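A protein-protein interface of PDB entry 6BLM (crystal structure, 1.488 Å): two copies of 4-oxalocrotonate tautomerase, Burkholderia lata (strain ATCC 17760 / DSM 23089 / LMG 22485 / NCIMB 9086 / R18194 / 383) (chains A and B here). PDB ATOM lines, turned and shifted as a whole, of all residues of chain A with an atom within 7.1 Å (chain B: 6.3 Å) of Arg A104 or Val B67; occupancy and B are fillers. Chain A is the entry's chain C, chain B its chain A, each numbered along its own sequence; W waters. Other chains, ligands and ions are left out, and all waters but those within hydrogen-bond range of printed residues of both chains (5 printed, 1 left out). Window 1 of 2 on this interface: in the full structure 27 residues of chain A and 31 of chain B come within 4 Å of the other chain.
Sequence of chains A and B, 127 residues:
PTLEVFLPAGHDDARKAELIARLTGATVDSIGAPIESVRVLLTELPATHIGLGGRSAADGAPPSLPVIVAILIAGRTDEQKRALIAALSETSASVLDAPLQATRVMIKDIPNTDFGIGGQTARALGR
Among the printed residues, pairs that only touch across the chains: Phe A6 with Val B69, Phe A6 with Met B106, Leu A52 with Thr B103, Leu A52 with Arg B104, Val A67 with Met B106, Ile A85 with Gly B51, Ile A85 with Gly B54, Ser A89 with Gly B54, Leu A100 with Gly B53, Gln A101 with Leu B52, Gln A101 with Gly B53, Ala A102 with Leu B52, Thr A103 with Gly B51, Thr A103 with Leu B52, Thr A103 with Gly B54, Arg A104 with Gly B51, Arg A104 with Leu B52, Arg A104 with Val B67, Met A106 with Phe B6, Met A106 with Leu B65 and Met A106 with Val B67.
NH2 of Arg A104 lies close to NH2 of Arg B104.
The backbone NH (N) of Gly B51 lies within hydrogen-bond range of the backbone carbonyl oxygen (O) of Val A105.
O of Ser B64 sits at hydrogen-bond distance from NH1 of Arg A104, at 2.5 Å.
N of Gly B53 sits at hydrogen-bond distance from O of Thr A103 (2.9 Å).
The backbone carbonyl oxygen (O) of Ala B102 sits at hydrogen-bond distance from the guanidinium group (NH2) of Arg A104 (2.8 Å).
Arg A104 touches Ala B102, but with the chains exchanged Ala A102 does not touch Arg B104 (5.5 Å).
Met A106 touches Leu B65, but with the chains exchanged Leu A65 does not touch Met B106 (5.4 Å).
Water W2 lies within hydrogen-bond range of the backbone carbonyl oxygen (O) of Ala A102 (2.7 Å), the guanidinium group (NE) of Arg A104 (2.9 Å) and the guanidinium group (NH2) of Arg B104 (3.0 Å).
Water W5 bridges NH2 of Arg A104 (3.1 Å) and O of Pro B63 (3.4 Å).
Ser A92 touches none of the printed residues of chain B.
Of the printed residues of chain B, Thr A103 touches Gly B51, Leu B52, Gly B53 and Gly B54.
Arg A104 touches just these residues of chain B: Gly B51 (3.3 Å), Leu B52 (3.8 Å), Ser B64 (2.5 Å), Val B67 (3.4 Å), Ala B102 (2.8 Å) and Arg B104 (3.3 Å).
Of the printed residues of chain A, Phe B6 touches Met A106.
Of the printed residues of chain A, Leu B65 touches Met A106 (3.8 Å).
Val B67 touches two residues of chain A.
Of the 20 printed residues of chain A, 12 touch a printed residue of chain B.
Hydrophobic or aromatic side chains of chain A that line the printed part of chain B: Phe A6, Leu A52, Val A67, Ile A85, Leu A100 and Met A106.
Printed residues of chain B that touch a printed residue of chain A: Phe B6, Gly B51, Leu B52, Gly B53, Gly B54, Ser B64, Leu B65, Val B67, Val B69, Ala B102, Thr B103, Arg B104 and Met B106.
Along chain B the printed residues that touch a printed residue of chain A span positions 6 to 106.
The backbone NH of Glu B4 is in hydrogen-bond range of the backbone carbonyl oxygen of Val B69 (2.8 Å).
The backbone NH (N) of Ile B68 sits at hydrogen-bond distance from the backbone carbonyl oxygen (O) of Arg B104 (2.8 Å).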
ATOM      1  N   PHE A   6       2.083  23.981  25.157  1.00  0.00           N
ATOM      2  CA  PHE A   6       2.524  23.008  24.173  1.00  0.00           C
ATOM      3  C   PHE A   6       3.136  23.792  23.038  1.00  0.00           C
ATOM      4  O   PHE A   6       2.458  24.606  22.397  1.00  0.00           O
ATOM      5  CB  PHE A   6       1.355  22.150  23.696  1.00  0.00           C
ATOM      6  CG  PHE A   6       0.851  21.185  24.732  1.00  0.00           C
ATOM      7  CD1 PHE A   6      -0.054  21.586  25.702  1.00  0.00           C
ATOM      8  CD2 PHE A   6       1.288  19.866  24.746  1.00  0.00           C
ATOM      9  CE1 PHE A   6      -0.506  20.701  26.662  1.00  0.00           C
ATOM     10  CE2 PHE A   6       0.829  18.977  25.707  1.00  0.00           C
ATOM     11  CZ  PHE A   6      -0.066  19.391  26.662  1.00  0.00           C
ATOM     12  N   LEU A  52      -2.134  18.747  13.427  1.00  0.00           N
ATOM     13  CA  LEU A  52      -3.120  19.777  13.139  1.00  0.00           C
ATOM     14  C   LEU A  52      -3.966  19.301  11.979  1.00  0.00           C
ATOM     15  O   LEU A  52      -3.434  19.016  10.906  1.00  0.00           O
ATOM     16  CB  LEU A  52      -2.464  21.109  12.782  1.00  0.00           C
ATOM     17  CG  LEU A  52      -1.540  21.779  13.794  1.00  0.00           C
ATOM     18  CD1 LEU A  52      -0.124  21.267  13.623  1.00  0.00           C
ATOM     19  CD2 LEU A  52      -1.602  23.299  13.637  1.00  0.00           C
ATOM     20  N   SER A  64       2.338  25.119  13.923  1.00  0.00           N
ATOM     21  CA  SER A  64       1.471  25.186  15.096  1.00  0.00           C
ATOM     22  C   SER A  64       1.738  26.388  15.992  1.00  0.00           C
ATOM     23  O   SER A  64       2.869  26.617  16.426  1.00  0.00           O
ATOM     24  CB  SER A  64       1.606  23.909  15.927  1.00  0.00           C
ATOM     25  OG  SER A  64       0.674  23.902  17.002  1.00  0.00           O
ATOM     26  N   LEU A  65       0.684  27.154  16.261  1.00  0.00           N
ATOM     27  CA  LEU A  65       0.714  28.118  17.350  1.00  0.00           C
ATOM     28  C   LEU A  65       0.794  27.310  18.630  1.00  0.00           C
ATOM     29  O   LEU A  65       0.459  26.123  18.632  1.00  0.00           O
ATOM     30  CB  LEU A  65      -0.530  29.016  17.350  1.00  0.00           C
ATOM     31  CG  LEU A  65      -0.495  30.399  16.694  1.00  0.00           C
ATOM     32  CD1 LEU A  65       0.301  31.368  17.552  1.00  0.00           C
ATOM     33  CD2 LEU A  65       0.080  30.310  15.293  1.00  0.00           C
ATOM     34  N   PRO A  66       1.257  27.932  19.719  1.00  0.00           N
ATOM     35  CA  PRO A  66       1.204  27.190  20.976  1.00  0.00           C
ATOM     36  C   PRO A  66      -0.228  26.860  21.331  1.00  0.00           C
ATOM     37  O   PRO A  66      -1.170  27.537  20.929  1.00  0.00           O
ATOM     38  CB  PRO A  66       1.791  28.164  21.998  1.00  0.00           C
ATOM     39  CG  PRO A  66       2.583  29.117  21.210  1.00  0.00           C
ATOM     40  CD  PRO A  66       1.909  29.241  19.877  1.00  0.00           C
ATOM     41  N   VAL A  67      -0.379  25.788  22.081  1.00  0.00           N
ATOM     42  CA  VAL A  67      -1.638  25.491  22.719  1.00  0.00           C
ATOM     43  C   VAL A  67      -1.391  25.599  24.203  1.00  0.00           C
ATOM     44  O   VAL A  67      -0.528  24.921  24.753  1.00  0.00           O
ATOM     45  CB  VAL A  67      -2.147  24.107  22.343  1.00  0.00           C
ATOM     46  CG1 VAL A  67      -3.404  23.786  23.101  1.00  0.00           C
ATOM     47  CG2 VAL A  67      -2.375  24.055  20.823  1.00  0.00           C
ATOM     48  N   ILE A  68      -2.103  26.512  24.849  1.00  0.00           N
ATOM     49  CA  ILE A  68      -1.906  26.742  26.266  1.00  0.00           C
ATOM     50  C   ILE A  68      -3.054  26.159  27.060  1.00  0.00           C
ATOM     51  O   ILE A  68      -4.212  26.498  26.811  1.00  0.00           O
ATOM     52  CB  ILE A  68      -1.807  28.240  26.586  1.00  0.00           C
ATOM     53  CG1 ILE A  68      -0.663  28.878  25.805  1.00  0.00           C
ATOM     54  CG2 ILE A  68      -1.625  28.430  28.086  1.00  0.00           C
ATOM     55  CD1 ILE A  68      -0.636  30.407  25.913  1.00  0.00           C
ATOM     56  N   VAL A  69      -2.737  25.268  27.997  1.00  0.00           N
ATOM     57  CA  VAL A  69      -3.720  24.815  28.973  1.00  0.00           C
ATOM     58  C   VAL A  69      -3.512  25.640  30.237  1.00  0.00           C
ATOM     59  O   VAL A  69      -2.432  25.618  30.827  1.00  0.00           O
ATOM     60  CB  VAL A  69      -3.593  23.316  29.266  1.00  0.00           C
ATOM     61  CG1 VAL A  69      -4.606  22.897  30.343  1.00  0.00           C
ATOM     62  CG2 VAL A  69      -3.818  22.538  27.962  1.00  0.00           C
ATOM     63  N   ILE A  85      -8.105  34.644  28.267  1.00  0.00           N
ATOM     64  CA  ILE A  85      -7.993  34.099  26.908  1.00  0.00           C
ATOM     65  C   ILE A  85      -7.437  35.165  25.955  1.00  0.00           C
ATOM     66  O   ILE A  85      -6.552  34.881  25.155  1.00  0.00           O
ATOM     67  CB  ILE A  85      -9.351  33.571  26.410  1.00  0.00           C
ATOM     68  CG1 ILE A  85      -9.694  32.263  27.134  1.00  0.00           C
ATOM     69  CG2 ILE A  85      -9.337  33.335  24.884  1.00  0.00           C
ATOM     70  CD1 ILE A  85     -11.111  31.769  26.883  1.00  0.00           C
ATOM     71  N   LEU A  88      -3.501  35.994  27.003  1.00  0.00           N
ATOM     72  CA  LEU A  88      -2.550  34.938  26.704  1.00  0.00           C
ATOM     73  C   LEU A  88      -2.413  34.757  25.203  1.00  0.00           C
ATOM     74  O   LEU A  88      -1.343  34.440  24.708  1.00  0.00           O
ATOM     75  CB  LEU A  88      -2.989  33.608  27.334  1.00  0.00           C
ATOM     76  CG  LEU A  88      -3.012  33.502  28.855  1.00  0.00           C
ATOM     77  CD1 LEU A  88      -3.471  32.097  29.249  1.00  0.00           C
ATOM     78  CD2 LEU A  88      -1.646  33.806  29.466  1.00  0.00           C
ATOM     79  N   SER A  89      -3.504  34.970  24.486  1.00  0.00           N
ATOM     80  CA  SER A  89      -3.496  34.782  23.036  1.00  0.00           C
ATOM     81  C   SER A  89      -2.741  35.902  22.316  1.00  0.00           C
ATOM     82  O   SER A  89      -1.895  35.641  21.471  1.00  0.00           O
ATOM     83  CB  SER A  89      -4.924  34.679  22.514  1.00  0.00           C
ATOM     84  OG  SER A  89      -5.590  33.572  23.117  1.00  0.00           O
ATOM     85  N   SER A  92       0.944  35.379  23.113  1.00  0.00           N
ATOM     86  CA  SER A  92       1.468  34.299  22.278  1.00  0.00           C
ATOM     87  C   SER A  92       1.730  34.747  20.839  1.00  0.00           C
ATOM     88  O   SER A  92       2.793  34.466  20.275  1.00  0.00           O
ATOM     89  CB  SER A  92       0.501  33.113  22.284  1.00  0.00           C
ATOM     90  OG  SER A  92       0.386  32.577  23.587  1.00  0.00           O
ATOM     91  N   PRO A  99       0.075  34.171  13.764  1.00  0.00           N
ATOM     92  CA  PRO A  99      -1.286  34.685  13.570  1.00  0.00           C
ATOM     93  C   PRO A  99      -2.121  34.617  14.841  1.00  0.00           C
ATOM     94  O   PRO A  99      -2.276  33.529  15.389  1.00  0.00           O
ATOM     95  CB  PRO A  99      -1.871  33.758  12.500  1.00  0.00           C
ATOM     96  CG  PRO A  99      -0.696  33.118  11.848  1.00  0.00           C
ATOM     97  CD  PRO A  99       0.352  33.011  12.899  1.00  0.00           C
ATOM     98  N   LEU A 100      -2.643  35.754  15.288  1.00  0.00           N
ATOM     99  CA  LEU A 100      -3.509  35.788  16.464  1.00  0.00           C
ATOM    100  C   LEU A 100      -4.689  34.847  16.272  1.00  0.00           C
ATOM    101  O   LEU A 100      -5.137  34.195  17.212  1.00  0.00           O
ATOM    102  CB  LEU A 100      -3.999  37.211  16.732  1.00  0.00           C
ATOM    103  CG  LEU A 100      -4.941  37.395  17.926  1.00  0.00           C
ATOM    104  CD1 LEU A 100      -4.255  37.000  19.224  1.00  0.00           C
ATOM    105  CD2 LEU A 100      -5.416  38.835  17.988  1.00  0.00           C
ATOM    106  N   GLN A 101      -5.159  34.760  15.034  1.00  0.00           N
ATOM    107  CA  GLN A 101      -6.321  33.955  14.676  1.00  0.00           C
ATOM    108  C   GLN A 101      -6.178  32.472  15.039  1.00  0.00           C
ATOM    109  O   GLN A 101      -7.181  31.778  15.265  1.00  0.00           O
ATOM    110  CB  GLN A 101      -6.589  34.091  13.175  1.00  0.00           C
ATOM    111  CG  GLN A 101      -6.898  35.518  12.715  1.00  0.00           C
ATOM    112  CD  GLN A 101      -5.652  36.383  12.474  1.00  0.00           C
ATOM    113  OE1 GLN A 101      -4.520  35.958  12.709  1.00  0.00           O
ATOM    114  NE2 GLN A 101      -5.871  37.602  11.988  1.00  0.00           N
ATOM    115  N   ALA A 102      -4.938  31.993  15.108  1.00  0.00           N
ATOM    116  CA  ALA A 102      -4.684  30.574  15.342  1.00  0.00           C
ATOM    117  C   ALA A 102      -4.267  30.251  16.774  1.00  0.00           C
ATOM    118  O   ALA A 102      -4.039  29.088  17.100  1.00  0.00           O
ATOM    119  CB  ALA A 102      -3.623  30.074  14.382  1.00  0.00           C
ATOM    120  N   THR A 103      -4.148  31.270  17.617  1.00  0.00           N
ATOM    121  CA  THR A 103      -3.771  31.065  19.026  1.00  0.00           C
ATOM    122  C   THR A 103      -4.841  30.285  19.797  1.00  0.00           C
ATOM    123  O   THR A 103      -6.028  30.427  19.538  1.00  0.00           O
ATOM    124  CB  THR A 103      -3.507  32.409  19.730  1.00  0.00           C
ATOM    125  OG1 THR A 103      -4.676  33.234  19.656  1.00  0.00           O
ATOM    126  CG2 THR A 103      -2.343  33.131  19.083  1.00  0.00           C
ATOM    127  N   ARG A 104      -4.404  29.437  20.727  1.00  0.00           N
ATOM    128  CA  ARG A 104      -5.309  28.558  21.475  1.00  0.00           C
ATOM    129  C   ARG A 104      -5.047  28.595  22.969  1.00  0.00           C
ATOM    130  O   ARG A 104      -3.908  28.480  23.415  1.00  0.00           O
ATOM    131  CB  ARG A 104      -5.180  27.107  20.989  1.00  0.00           C
ATOM    132  CG  ARG A 104      -5.913  26.833  19.697  1.00  0.00           C
ATOM    133  CD  ARG A 104      -5.436  25.536  19.091  1.00  0.00           C
ATOM    134  NE  ARG A 104      -6.187  25.196  17.877  1.00  0.00           N
ATOM    135  CZ  ARG A 104      -7.205  24.340  17.840  1.00  0.00           C
ATOM    136  NH1 ARG A 104      -7.606  23.708  18.944  1.00  0.00           N
ATOM    137  NH2 ARG A 104      -7.815  24.100  16.681  1.00  0.00           N
ATOM    138  N   VAL A 105      -6.120  28.763  23.727  1.00  0.00           N
ATOM    139  CA  VAL A 105      -6.092  28.694  25.184  1.00  0.00           C
ATOM    140  C   VAL A 105      -7.240  27.830  25.659  1.00  0.00           C
ATOM    141  O   VAL A 105      -8.370  28.027  25.230  1.00  0.00           O
ATOM    142  CB  VAL A 105      -6.218  30.098  25.811  1.00  0.00           C
ATOM    143  CG1 VAL A 105      -6.312  30.001  27.315  1.00  0.00           C
ATOM    144  CG2 VAL A 105      -5.039  30.958  25.401  1.00  0.00           C
ATOM    145  N   MET A 106      -6.961  26.850  26.519  1.00  0.00           N
ATOM    146  CA  MET A 106      -8.015  26.043  27.125  1.00  0.00           C
ATOM    147  C   MET A 106      -7.917  26.173  28.636  1.00  0.00           C
ATOM    148  O   MET A 106      -6.885  25.867  29.219  1.00  0.00           O
ATOM    149  CB  MET A 106      -7.923  24.574  26.687  1.00  0.00           C
ATOM    150  CG  MET A 106      -7.976  24.428  25.156  1.00  0.00           C
ATOM    151  SD  MET A 106      -8.014  22.707  24.613  1.00  0.00           S
ATOM    152  CE  MET A 106      -6.432  22.140  25.227  1.00  0.00           C
ATOM    153  N   GLU B   4      -5.922  12.133  26.757  1.00  0.00           N
ATOM    154  CA  GLU B   4      -6.844  13.116  27.332  1.00  0.00           C
ATOM    155  C   GLU B   4      -7.481  13.890  26.183  1.00  0.00           C
ATOM    156  O   GLU B   4      -6.780  14.456  25.334  1.00  0.00           O
ATOM    157  CB  GLU B   4      -6.135  14.063  28.305  1.00  0.00           C
ATOM    158  CG  GLU B   4      -7.091  15.140  28.860  1.00  0.00           C
ATOM    159  CD  GLU B   4      -6.468  16.014  29.936  1.00  0.00           C
ATOM    160  OE1 GLU B   4      -5.226  16.024  30.050  1.00  0.00           O
ATOM    161  OE2 GLU B   4      -7.231  16.719  30.641  1.00  0.00           O
ATOM    162  N   VAL B   5      -8.807  13.879  26.128  1.00  0.00           N
ATOM    163  CA  VAL B   5      -9.548  14.506  25.046  1.00  0.00           C
ATOM    164  C   VAL B   5     -10.278  15.722  25.590  1.00  0.00           C
ATOM    165  O   VAL B   5     -11.178  15.572  26.420  1.00  0.00           O
ATOM    166  CB  VAL B   5     -10.591  13.536  24.431  1.00  0.00           C
ATOM    167  CG1 VAL B   5     -11.276  14.164  23.224  1.00  0.00           C
ATOM    168  CG2 VAL B   5      -9.925  12.207  24.067  1.00  0.00           C
ATOM    169  N   PHE B   6      -9.868  16.909  25.163  1.00  0.00           N
ATOM    170  CA  PHE B   6     -10.608  18.138  25.470  1.00  0.00           C
ATOM    171  C   PHE B   6     -11.748  18.265  24.464  1.00  0.00           C
ATOM    172  O   PHE B   6     -11.514  18.283  23.242  1.00  0.00           O
ATOM    173  CB  PHE B   6      -9.686  19.355  25.401  1.00  0.00           C
ATOM    174  CG  PHE B   6      -8.580  19.331  26.405  1.00  0.00           C
ATOM    175  CD1 PHE B   6      -7.378  18.689  26.134  1.00  0.00           C
ATOM    176  CD2 PHE B   6      -8.753  19.945  27.645  1.00  0.00           C
ATOM    177  CE1 PHE B   6      -6.357  18.681  27.082  1.00  0.00           C
ATOM    178  CE2 PHE B   6      -7.737  19.926  28.598  1.00  0.00           C
ATOM    179  CZ  PHE B   6      -6.544  19.289  28.315  1.00  0.00           C
ATOM    180  N   LEU B   7     -12.977  18.344  24.968  1.00  0.00           N
ATOM    181  CA  LEU B   7     -14.160  18.401  24.111  1.00  0.00           C
ATOM    182  C   LEU B   7     -15.186  19.329  24.742  1.00  0.00           C
ATOM    183  O   LEU B   7     -15.138  19.582  25.947  1.00  0.00           O
ATOM    184  CB  LEU B   7     -14.754  16.992  23.891  1.00  0.00           C
ATOM    185  CG  LEU B   7     -15.565  16.341  25.021  1.00  0.00           C
ATOM    186  CD1 LEU B   7     -16.286  15.086  24.484  1.00  0.00           C
ATOM    187  CD2 LEU B   7     -14.666  15.959  26.187  1.00  0.00           C
ATOM    188  N   GLY B  51     -10.707  28.675  23.945  1.00  0.00           N
ATOM    189  CA  GLY B  51     -10.229  29.868  23.262  1.00  0.00           C
ATOM    190  C   GLY B  51      -9.530  29.589  21.946  1.00  0.00           C
ATOM    191  O   GLY B  51      -8.627  28.754  21.862  1.00  0.00           O
ATOM    192  N   LEU B  52      -9.952  30.314  20.913  1.00  0.00           N
ATOM    193  CA  LEU B  52      -9.277  30.320  19.621  1.00  0.00           C
ATOM    194  C   LEU B  52      -9.286  31.754  19.105  1.00  0.00           C
ATOM    195  O   LEU B  52     -10.327  32.403  19.084  1.00  0.00           O
ATOM    196  CB  LEU B  52      -9.964  29.388  18.619  1.00  0.00           C
ATOM    197  CG  LEU B  52      -9.430  29.384  17.183  1.00  0.00           C
ATOM    198  CD1 LEU B  52      -8.028  28.804  17.161  1.00  0.00           C
ATOM    199  CD2 LEU B  52     -10.357  28.597  16.259  1.00  0.00           C
ATOM    200  N   GLY B  53      -8.124  32.243  18.714  1.00  0.00           N
ATOM    201  CA  GLY B  53      -8.024  33.604  18.197  1.00  0.00           C
ATOM    202  C   GLY B  53      -8.192  34.668  19.264  1.00  0.00           C
ATOM    203  O   GLY B  53      -8.424  35.833  18.948  1.00  0.00           O
ATOM    204  N   GLY B  54      -8.073  34.278  20.528  1.00  0.00           N
ATOM    205  CA  GLY B  54      -8.224  35.230  21.626  1.00  0.00           C
ATOM    206  C   GLY B  54      -9.651  35.462  22.058  1.00  0.00           C
ATOM    207  O   GLY B  54      -9.907  36.348  22.876  1.00  0.00           O
ATOM    208  N   PRO B  63     -14.790  26.638  15.537  1.00  0.00           N
ATOM    209  CA  PRO B  63     -14.500  25.340  16.166  1.00  0.00           C
ATOM    210  C   PRO B  63     -13.006  25.121  16.415  1.00  0.00           C
ATOM    211  O   PRO B  63     -12.169  25.437  15.557  1.00  0.00           O
ATOM    212  CB  PRO B  63     -15.027  24.332  15.145  1.00  0.00           C
ATOM    213  CG  PRO B  63     -16.120  25.062  14.418  1.00  0.00           C
ATOM    214  CD  PRO B  63     -15.669  26.502  14.359  1.00  0.00           C
ATOM    215  N   SER B  64     -12.676  24.581  17.585  1.00  0.00           N
ATOM    216  CA  SER B  64     -11.284  24.366  17.950  1.00  0.00           C
ATOM    217  C   SER B  64     -11.066  23.058  18.712  1.00  0.00           C
ATOM    218  O   SER B  64      -9.935  22.734  19.069  1.00  0.00           O
ATOM    219  CB  SER B  64     -10.772  25.535  18.792  1.00  0.00           C
ATOM    220  OG  SER B  64     -11.430  25.587  20.053  1.00  0.00           O
ATOM    221  N   LEU B  65     -12.141  22.329  18.977  1.00  0.00           N
ATOM    222  CA  LEU B  65     -12.045  21.031  19.649  1.00  0.00           C
ATOM    223  C   LEU B  65     -12.543  19.917  18.706  1.00  0.00           C
ATOM    224  O   LEU B  65     -13.309  20.195  17.793  1.00  0.00           O
ATOM    225  CB  LEU B  65     -12.858  21.056  20.957  1.00  0.00           C
ATOM    226  CG  LEU B  65     -12.442  22.107  21.993  1.00  0.00           C
ATOM    227  CD1 LEU B  65     -13.215  21.866  23.248  1.00  0.00           C
ATOM    228  CD2 LEU B  65     -10.944  22.022  22.250  1.00  0.00           C
ATOM    229  N   PRO B  66     -12.135  18.649  18.932  1.00  0.00           N
ATOM    230  CA  PRO B  66     -11.331  18.116  20.036  1.00  0.00           C
ATOM    231  C   PRO B  66      -9.830  18.308  19.904  1.00  0.00           C
ATOM    232  O   PRO B  66      -9.275  18.353  18.809  1.00  0.00           O
ATOM    233  CB  PRO B  66     -11.670  16.623  20.025  1.00  0.00           C
ATOM    234  CG  PRO B  66     -12.021  16.347  18.576  1.00  0.00           C
ATOM    235  CD  PRO B  66     -12.713  17.577  18.094  1.00  0.00           C
ATOM    236  N   VAL B  67      -9.188  18.422  21.062  1.00  0.00           N
ATOM    237  CA  VAL B  67      -7.742  18.443  21.203  1.00  0.00           C
ATOM    238  C   VAL B  67      -7.375  17.226  22.048  1.00  0.00           C
ATOM    239  O   VAL B  67      -7.976  16.991  23.101  1.00  0.00           O
ATOM    240  CB  VAL B  67      -7.247  19.746  21.884  1.00  0.00           C
ATOM    241  CG1 VAL B  67      -5.772  19.648  22.245  1.00  0.00           C
ATOM    242  CG2 VAL B  67      -7.559  20.977  21.003  1.00  0.00           C
ATOM    243  N   ILE B  68      -6.438  16.418  21.559  1.00  0.00           N
ATOM    244  CA  ILE B  68      -6.096  15.174  22.242  1.00  0.00           C
ATOM    245  C   ILE B  68      -4.625  15.179  22.628  1.00  0.00           C
ATOM    246  O   ILE B  68      -3.755  15.404  21.779  1.00  0.00           O
ATOM    247  CB  ILE B  68      -6.401  13.964  21.354  1.00  0.00           C
ATOM    248  CG1 ILE B  68      -7.881  13.973  20.977  1.00  0.00           C
ATOM    249  CG2 ILE B  68      -6.036  12.657  22.077  1.00  0.00           C
ATOM    250  CD1 ILE B  68      -8.280  12.853  20.024  1.00  0.00           C
ATOM    251  N   VAL B  69      -4.359  14.953  23.905  1.00  0.00           N
ATOM    252  CA  VAL B  69      -2.991  14.759  24.388  1.00  0.00           C
ATOM    253  C   VAL B  69      -2.789  13.263  24.595  1.00  0.00           C
ATOM    254  O   VAL B  69      -3.537  12.626  25.339  1.00  0.00           O
ATOM    255  CB  VAL B  69      -2.716  15.523  25.693  1.00  0.00           C
ATOM    256  CG1 VAL B  69      -1.313  15.202  26.203  1.00  0.00           C
ATOM    257  CG2 VAL B  69      -2.903  17.035  25.488  1.00  0.00           C
ATOM    258  N   GLN B 101     -10.220  20.119  10.560  1.00  0.00           N
ATOM    259  CA  GLN B 101      -9.200  21.141  10.710  1.00  0.00           C
ATOM    260  C   GLN B 101      -9.128  21.700  12.134  1.00  0.00           C
ATOM    261  O   GLN B 101      -8.104  22.264  12.517  1.00  0.00           O
ATOM    262  CB  GLN B 101      -9.437  22.284   9.719  1.00  0.00           C
ATOM    263  CG  GLN B 101      -8.752  22.093   8.366  1.00  0.00           C
ATOM    264  CD  GLN B 101      -7.552  21.153   8.413  1.00  0.00           C
ATOM    265  OE1 GLN B 101      -7.661  19.964   8.096  1.00  0.00           O
ATOM    266  NE2 GLN B 101      -6.397  21.687   8.796  1.00  0.00           N
ATOM    267  N   ALA B 102     -10.197  21.533  12.908  1.00  0.00           N
ATOM    268  CA  ALA B 102     -10.224  22.015  14.297  1.00  0.00           C
ATOM    269  C   ALA B 102      -9.396  21.110  15.213  1.00  0.00           C
ATOM    270  O   ALA B 102      -8.947  21.533  16.279  1.00  0.00           O
ATOM    271  CB  ALA B 102     -11.650  22.112  14.818  1.00  0.00           C
ATOM    272  N   THR B 103      -9.189  19.864  14.807  1.00  0.00           N
ATOM    273  CA  THR B 103      -8.577  18.895  15.720  1.00  0.00           C
ATOM    274  C   THR B 103      -7.078  19.130  15.908  1.00  0.00           C
ATOM    275  O   THR B 103      -6.368  19.560  14.991  1.00  0.00           O
ATOM    276  CB  THR B 103      -8.783  17.426  15.237  1.00  0.00           C
ATOM    277  OG1 THR B 103      -8.056  17.197  14.021  1.00  0.00           O
ATOM    278  CG2 THR B 103     -10.260  17.138  15.004  1.00  0.00           C
ATOM    279  N   ARG B 104      -6.595  18.829  17.108  1.00  0.00           N
ATOM    280  CA  ARG B 104      -5.166  18.886  17.400  1.00  0.00           C
ATOM    281  C   ARG B 104      -4.797  17.634  18.168  1.00  0.00           C
ATOM    282  O   ARG B 104      -5.604  17.148  18.956  1.00  0.00           O
ATOM    283  CB  ARG B 104      -4.792  20.121  18.249  1.00  0.00           C
ATOM    284  CG  ARG B 104      -5.101  21.447  17.609  1.00  0.00           C
ATOM    285  CD  ARG B 104      -4.126  21.720  16.496  1.00  0.00           C
ATOM    286  NE  ARG B 104      -4.351  23.026  15.877  1.00  0.00           N
ATOM    287  CZ  ARG B 104      -5.194  23.234  14.864  1.00  0.00           C
ATOM    288  NH1 ARG B 104      -5.901  22.230  14.365  1.00  0.00           N
ATOM    289  NH2 ARG B 104      -5.335  24.451  14.352  1.00  0.00           N
ATOM    290  N   VAL B 105      -3.594  17.118  17.925  1.00  0.00           N
ATOM    291  CA  VAL B 105      -3.051  16.014  18.697  1.00  0.00           C
ATOM    292  C   VAL B 105      -1.660  16.395  19.166  1.00  0.00           C
ATOM    293  O   VAL B 105      -0.880  16.958  18.405  1.00  0.00           O
ATOM    294  CB  VAL B 105      -3.001  14.730  17.856  1.00  0.00           C
ATOM    295  CG1 VAL B 105      -2.317  13.580  18.632  1.00  0.00           C
ATOM    296  CG2 VAL B 105      -4.400  14.342  17.401  1.00  0.00           C
ATOM    297  N   MET B 106      -1.363  16.113  20.425  1.00  0.00           N
ATOM    298  CA  MET B 106      -0.037  16.339  20.988  1.00  0.00           C
ATOM    299  C   MET B 106       0.437  15.057  21.601  1.00  0.00           C
ATOM    300  O   MET B 106      -0.177  14.576  22.546  1.00  0.00           O
ATOM    301  CB  MET B 106      -0.059  17.415  22.066  1.00  0.00           C
ATOM    302  CG  MET B 106      -0.711  18.698  21.656  1.00  0.00           C
ATOM    303  SD  MET B 106       0.411  19.621  20.643  1.00  0.00           S
ATOM    304  CE  MET B 106      -0.375  21.227  20.661  1.00  0.00           C
HETATM  305  O   HOH W   1      -2.539  24.657  16.987  1.00  0.00           O
HETATM  306  O   HOH W   2      -5.149  27.013  15.804  1.00  0.00           O
HETATM  307  O   HOH W   3      -3.641  19.796   8.253  1.00  0.00           O
HETATM  308  O   HOH W   4      -4.923  16.841  14.307  1.00  0.00           O
HETATM  309  O   HOH W   5      -9.017  25.403  14.185  1.00  0.00           O
